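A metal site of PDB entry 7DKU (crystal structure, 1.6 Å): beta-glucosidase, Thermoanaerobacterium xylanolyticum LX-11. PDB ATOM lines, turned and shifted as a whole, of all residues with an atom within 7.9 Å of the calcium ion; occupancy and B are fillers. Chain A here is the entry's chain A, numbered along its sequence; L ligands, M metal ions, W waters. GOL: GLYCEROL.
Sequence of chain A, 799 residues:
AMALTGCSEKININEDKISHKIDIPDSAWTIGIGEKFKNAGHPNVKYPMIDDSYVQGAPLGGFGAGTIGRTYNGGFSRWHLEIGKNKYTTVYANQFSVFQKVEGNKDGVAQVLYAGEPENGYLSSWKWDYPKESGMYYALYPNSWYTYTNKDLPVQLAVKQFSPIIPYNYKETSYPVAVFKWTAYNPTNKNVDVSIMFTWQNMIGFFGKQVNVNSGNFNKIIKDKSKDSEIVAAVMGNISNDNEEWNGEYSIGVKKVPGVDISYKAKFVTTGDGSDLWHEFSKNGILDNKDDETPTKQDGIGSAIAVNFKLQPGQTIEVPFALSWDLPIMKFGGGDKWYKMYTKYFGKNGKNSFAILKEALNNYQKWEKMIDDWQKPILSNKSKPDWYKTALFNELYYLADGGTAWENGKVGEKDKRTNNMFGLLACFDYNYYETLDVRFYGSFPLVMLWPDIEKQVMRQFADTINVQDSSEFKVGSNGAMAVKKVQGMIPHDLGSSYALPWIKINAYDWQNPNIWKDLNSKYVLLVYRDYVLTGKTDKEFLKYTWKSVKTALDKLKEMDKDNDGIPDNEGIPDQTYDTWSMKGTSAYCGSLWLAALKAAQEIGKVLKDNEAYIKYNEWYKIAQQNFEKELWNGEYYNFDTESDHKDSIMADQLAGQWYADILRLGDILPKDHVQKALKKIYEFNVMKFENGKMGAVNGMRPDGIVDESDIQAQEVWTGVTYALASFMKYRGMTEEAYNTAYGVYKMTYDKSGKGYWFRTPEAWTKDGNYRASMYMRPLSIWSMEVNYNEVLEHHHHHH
OD1 of Asp 568 lies close to N of Lys 561, 2.9 Å away.
The backbone NH (N) of Asp 568 sits at hydrogen-bond distance from the backbone carbonyl oxygen (O) of Met 559 (3.0 Å).
OG1 of Thr 585 lies within hydrogen-bond range of OD2 of Asp 564, 3.0 Å away.
The side-chain carboxylate of Asp 564 lies close to the side-chain carboxylate of Glu 630 (2.7 Å).
The side-chain amide nitrogen (ND2) of Asn 626 lies within hydrogen-bond range of the backbone carbonyl oxygen (O) of Asp 564 (2.8 Å).
OD2 of Asp 560 lies close to N of Asn 563, 3.5 Å away.
The backbone NH (N) of Gly 565 sits at hydrogen-bond distance from the side-chain carboxylate (OD2) of Asp 560 (2.8 Å).
Along chain A the residues within 4 Å of the calcium ion span positions 560 to 568.
The nearest printed residue that does not touch the calcium ion is Lys 561 (4.2 Å).
Water W1 lies within hydrogen-bond range of the side-chain hydroxyl of Thr 585 and the backbone carbonyl oxygen of Pro 567.
The calcium ion is bound by OD1 of Asp 568 (2.2 Å), OD1 of Asp 564 (2.3 Å), O of Ile 566 (2.4 Å), OD1 of Asp 560 (2.4 Å), OD1 of Asp 562 (2.4 Å), water W1 (2.4 Å) and O3 of the ligand (2.8 Å).
The calcium ion has seven donor atoms within binding distance.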
ATOM      1  N   LYS A 557      -4.669  18.920  11.626  1.00  0.00           N
ATOM      2  CA  LYS A 557      -5.837  19.771  11.372  1.00  0.00           C
ATOM      3  C   LYS A 557      -6.663  19.271  10.196  1.00  0.00           C
ATOM      4  O   LYS A 557      -7.889  19.349  10.235  1.00  0.00           O
ATOM      5  CB  LYS A 557      -5.399  21.213  11.123  1.00  0.00           C
ATOM      6  CG  LYS A 557      -6.528  22.227  10.922  1.00  0.00           C
ATOM      7  CD  LYS A 557      -7.498  22.253  12.093  1.00  0.00           C
ATOM      8  CE  LYS A 557      -8.157  23.611  12.283  1.00  0.00           C
ATOM      9  NZ  LYS A 557      -8.995  23.982  11.122  1.00  0.00           N
ATOM     10  N   MET A 559      -7.366  16.320   9.442  1.00  0.00           N
ATOM     11  CA  MET A 559      -8.215  15.210   9.897  1.00  0.00           C
ATOM     12  C   MET A 559      -9.479  15.635  10.658  1.00  0.00           C
ATOM     13  O   MET A 559     -10.224  14.794  11.135  1.00  0.00           O
ATOM     14  CB  MET A 559      -7.398  14.228  10.743  1.00  0.00           C
ATOM     15  CG  MET A 559      -6.298  13.537   9.974  1.00  0.00           C
ATOM     16  SD  MET A 559      -5.106  12.788  11.086  1.00  0.00           S
ATOM     17  CE  MET A 559      -4.022  12.008   9.887  1.00  0.00           C
ATOM     18  N   ASP A 560      -9.730  16.941  10.749  1.00  0.00           N
ATOM     19  CA  ASP A 560     -11.017  17.429  11.242  1.00  0.00           C
ATOM     20  C   ASP A 560     -12.037  17.254  10.109  1.00  0.00           C
ATOM     21  O   ASP A 560     -11.943  17.938   9.111  1.00  0.00           O
ATOM     22  CB  ASP A 560     -10.890  18.897  11.650  1.00  0.00           C
ATOM     23  CG  ASP A 560     -12.202  19.515  12.123  1.00  0.00           C
ATOM     24  OD1 ASP A 560     -13.181  18.799  12.428  1.00  0.00           O
ATOM     25  OD2 ASP A 560     -12.237  20.751  12.184  1.00  0.00           O
ATOM     26  N   LYS A 561     -12.985  16.344  10.292  1.00  0.00           N
ATOM     27  CA  LYS A 561     -13.992  16.016   9.257  1.00  0.00           C
ATOM     28  C   LYS A 561     -15.206  16.938   9.239  1.00  0.00           C
ATOM     29  O   LYS A 561     -15.870  17.040   8.206  1.00  0.00           O
ATOM     30  CB  LYS A 561     -14.501  14.578   9.442  1.00  0.00           C
ATOM     31  CG  LYS A 561     -13.499  13.494   9.082  1.00  0.00           C
ATOM     32  CD  LYS A 561     -14.047  12.137   9.492  1.00  0.00           C
ATOM     33  CE  LYS A 561     -13.219  10.982   8.953  1.00  0.00           C
ATOM     34  NZ  LYS A 561     -13.729   9.697   9.482  1.00  0.00           N
ATOM     35  N   ASP A 562     -15.503  17.590  10.355  1.00  0.00           N
ATOM     36  CA  ASP A 562     -16.762  18.340  10.508  1.00  0.00           C
ATOM     37  C   ASP A 562     -16.584  19.800  10.901  1.00  0.00           C
ATOM     38  O   ASP A 562     -17.536  20.444  11.348  1.00  0.00           O
ATOM     39  CB  ASP A 562     -17.665  17.619  11.509  1.00  0.00           C
ATOM     40  CG  ASP A 562     -17.082  17.596  12.905  1.00  0.00           C
ATOM     41  OD1 ASP A 562     -15.853  17.848  13.069  1.00  0.00           O
ATOM     42  OD2 ASP A 562     -17.840  17.340  13.856  1.00  0.00           O
ATOM     43  N   ASN A 563     -15.376  20.319  10.731  1.00  0.00           N
ATOM     44  CA  ASN A 563     -15.054  21.720  11.019  1.00  0.00           C
ATOM     45  C   ASN A 563     -15.442  22.185  12.437  1.00  0.00           C
ATOM     46  O   ASN A 563     -15.864  23.328  12.620  1.00  0.00           O
ATOM     47  CB  ASN A 563     -15.662  22.641   9.936  1.00  0.00           C
ATOM     48  CG  ASN A 563     -15.023  24.035   9.916  1.00  0.00           C
ATOM     49  OD1 ASN A 563     -13.839  24.195  10.220  1.00  0.00           O
ATOM     50  ND2 ASN A 563     -15.817  25.043   9.572  1.00  0.00           N
ATOM     51  N   ASP A 564     -15.274  21.324  13.437  1.00  0.00           N
ATOM     52  CA  ASP A 564     -15.348  21.772  14.829  1.00  0.00           C
ATOM     53  C   ASP A 564     -13.963  22.216  15.359  1.00  0.00           C
ATOM     54  O   ASP A 564     -13.841  22.608  16.509  1.00  0.00           O
ATOM     55  CB  ASP A 564     -16.011  20.715  15.738  1.00  0.00           C
ATOM     56  CG  ASP A 564     -15.077  19.567  16.103  1.00  0.00           C
ATOM     57  OD1 ASP A 564     -14.075  19.344  15.409  1.00  0.00           O
ATOM     58  OD2 ASP A 564     -15.371  18.862  17.084  1.00  0.00           O
ATOM     59  N   GLY A 565     -12.949  22.163  14.495  1.00  0.00           N
ATOM     60  CA  GLY A 565     -11.595  22.586  14.852  1.00  0.00           C
ATOM     61  C   GLY A 565     -10.745  21.501  15.508  1.00  0.00           C
ATOM     62  O   GLY A 565      -9.627  21.789  15.921  1.00  0.00           O
ATOM     63  N   ILE A 566     -11.274  20.279  15.589  1.00  0.00           N
ATOM     64  CA  ILE A 566     -10.608  19.168  16.288  1.00  0.00           C
ATOM     65  C   ILE A 566     -10.506  17.945  15.364  1.00  0.00           C
ATOM     66  O   ILE A 566     -11.496  17.577  14.719  1.00  0.00           O
ATOM     67  CB  ILE A 566     -11.370  18.788  17.580  1.00  0.00           C
ATOM     68  CG1 ILE A 566     -11.631  20.036  18.443  1.00  0.00           C
ATOM     69  CG2 ILE A 566     -10.589  17.754  18.387  1.00  0.00           C
ATOM     70  CD1 ILE A 566     -12.607  19.828  19.578  1.00  0.00           C
ATOM     71  N   PRO A 567      -9.323  17.308  15.289  1.00  0.00           N
ATOM     72  CA  PRO A 567      -9.281  16.077  14.501  1.00  0.00           C
ATOM     73  C   PRO A 567     -10.298  15.031  14.978  1.00  0.00           C
ATOM     74  O   PRO A 567     -10.600  14.962  16.165  1.00  0.00           O
ATOM     75  CB  PRO A 567      -7.849  15.561  14.686  1.00  0.00           C
ATOM     76  CG  PRO A 567      -7.329  16.253  15.888  1.00  0.00           C
ATOM     77  CD  PRO A 567      -8.041  17.570  15.967  1.00  0.00           C
ATOM     78  N   ASP A 568     -10.844  14.265  14.035  1.00  0.00           N
ATOM     79  CA  ASP A 568     -11.854  13.264  14.321  1.00  0.00           C
ATOM     80  C   ASP A 568     -11.220  11.886  14.440  1.00  0.00           C
ATOM     81  O   ASP A 568     -10.656  11.400  13.471  1.00  0.00           O
ATOM     82  CB  ASP A 568     -12.891  13.197  13.188  1.00  0.00           C
ATOM     83  CG  ASP A 568     -13.856  14.355  13.218  1.00  0.00           C
ATOM     84  OD1 ASP A 568     -13.442  15.510  12.996  1.00  0.00           O
ATOM     85  OD2 ASP A 568     -15.048  14.109  13.459  1.00  0.00           O
ATOM     86  N   ASN A 569     -11.374  11.234  15.585  1.00  0.00           N
ATOM     87  CA  ASN A 569     -11.047   9.802  15.687  1.00  0.00           C
ATOM     88  C   ASN A 569     -12.015   9.045  14.776  1.00  0.00           C
ATOM     89  O   ASN A 569     -13.179   9.449  14.640  1.00  0.00           O
ATOM     90  CB  ASN A 569     -11.120   9.308  17.134  1.00  0.00           C
ATOM     91  CG  ASN A 569     -10.047   9.919  18.027  1.00  0.00           C
ATOM     92  OD1 ASN A 569     -10.287  10.888  18.734  1.00  0.00           O
ATOM     93  ND2 ASN A 569      -8.865   9.314  18.007  1.00  0.00           N
ATOM     94  N   GLY A 584     -15.052  10.426  16.683  1.00  0.00           N
ATOM     95  CA  GLY A 584     -15.452  11.817  16.828  1.00  0.00           C
ATOM     96  C   GLY A 584     -14.397  12.578  17.591  1.00  0.00           C
ATOM     97  O   GLY A 584     -13.204  12.369  17.363  1.00  0.00           O
ATOM     98  N   THR A 585     -14.819  13.472  18.482  1.00  0.00           N
ATOM     99  CA  THR A 585     -13.891  14.185  19.350  1.00  0.00           C
ATOM    100  C   THR A 585     -13.718  13.334  20.584  1.00  0.00           C
ATOM    101  O   THR A 585     -14.703  12.995  21.227  1.00  0.00           O
ATOM    102  CB  THR A 585     -14.425  15.573  19.727  1.00  0.00           C
ATOM    103  OG1 THR A 585     -14.489  16.389  18.554  1.00  0.00           O
ATOM    104  CG2 THR A 585     -13.505  16.258  20.741  1.00  0.00           C
ATOM    105  N   ASN A 626     -15.256  24.181  21.516  1.00  0.00           N
ATOM    106  CA  ASN A 626     -16.000  23.026  21.038  1.00  0.00           C
ATOM    107  C   ASN A 626     -15.725  21.762  21.852  1.00  0.00           C
ATOM    108  O   ASN A 626     -16.631  20.963  22.070  1.00  0.00           O
ATOM    109  CB  ASN A 626     -15.769  22.822  19.540  1.00  0.00           C
ATOM    110  CG  ASN A 626     -16.462  23.893  18.704  1.00  0.00           C
ATOM    111  OD1 ASN A 626     -17.460  24.470  19.146  1.00  0.00           O
ATOM    112  ND2 ASN A 626     -15.943  24.164  17.513  1.00  0.00           N
ATOM    113  N   GLU A 630     -18.746  19.867  23.629  1.00  0.00           N
ATOM    114  CA  GLU A 630     -19.006  18.497  23.202  1.00  0.00           C
ATOM    115  C   GLU A 630     -18.866  17.453  24.295  1.00  0.00           C
ATOM    116  O   GLU A 630     -19.556  16.443  24.264  1.00  0.00           O
ATOM    117  CB  GLU A 630     -18.072  18.111  22.061  1.00  0.00           C
ATOM    118  CG  GLU A 630     -18.397  18.813  20.750  1.00  0.00           C
ATOM    119  CD  GLU A 630     -17.259  18.774  19.757  1.00  0.00           C
ATOM    120  OE1 GLU A 630     -16.321  17.960  19.939  1.00  0.00           O
ATOM    121  OE2 GLU A 630     -17.294  19.555  18.793  1.00  0.00           O
ATOM    122  N   THR A 641     -17.354  11.564  21.454  1.00  0.00           N
ATOM    123  CA  THR A 641     -18.689  12.038  21.050  1.00  0.00           C
ATOM    124  C   THR A 641     -19.539  11.031  20.290  1.00  0.00           C
ATOM    125  O   THR A 641     -20.750  11.242  20.181  1.00  0.00           O
ATOM    126  CB  THR A 641     -18.579  13.325  20.206  1.00  0.00           C
ATOM    127  OG1 THR A 641     -17.753  13.075  19.055  1.00  0.00           O
ATOM    128  CG2 THR A 641     -18.006  14.448  21.031  1.00  0.00           C
ATOM    129  N   GLU A 642     -18.944   9.959  19.772  1.00  0.00           N
ATOM    130  CA  GLU A 642     -19.647   9.046  18.856  1.00  0.00           C
ATOM    131  C   GLU A 642     -19.638   7.536  19.160  1.00  0.00           C
ATOM    132  O   GLU A 642     -20.391   6.779  18.532  1.00  0.00           O
ATOM    133  CB  GLU A 642     -19.164   9.304  17.424  1.00  0.00           C
ATOM    134  CG  GLU A 642     -19.501  10.695  16.923  1.00  0.00           C
ATOM    135  CD  GLU A 642     -19.099  10.939  15.482  1.00  0.00           C
ATOM    136  OE1 GLU A 642     -19.246  10.002  14.650  1.00  0.00           O
ATOM    137  OE2 GLU A 642     -18.662  12.054  15.159  1.00  0.00           O
HETATM  138  C1  GOL L   1     -18.161  16.375  17.551  1.00  0.00           C
HETATM  139  O1  GOL L   1     -19.521  16.561  17.996  1.00  0.00           O
HETATM  140  C2  GOL L   1     -18.166  15.356  16.406  1.00  0.00           C
HETATM  141  O2  GOL L   1     -18.628  14.099  16.898  1.00  0.00           O
HETATM  142  C3  GOL L   1     -16.786  15.106  15.801  1.00  0.00           C
HETATM  143  O3  GOL L   1     -16.022  16.263  15.471  1.00  0.00           O
HETATM  144 CA    CA M   1     -13.787  17.330  14.252  1.00  0.00          CA
HETATM  145  O   HOH W   1     -13.414  15.919  16.212  1.00  0.00           O
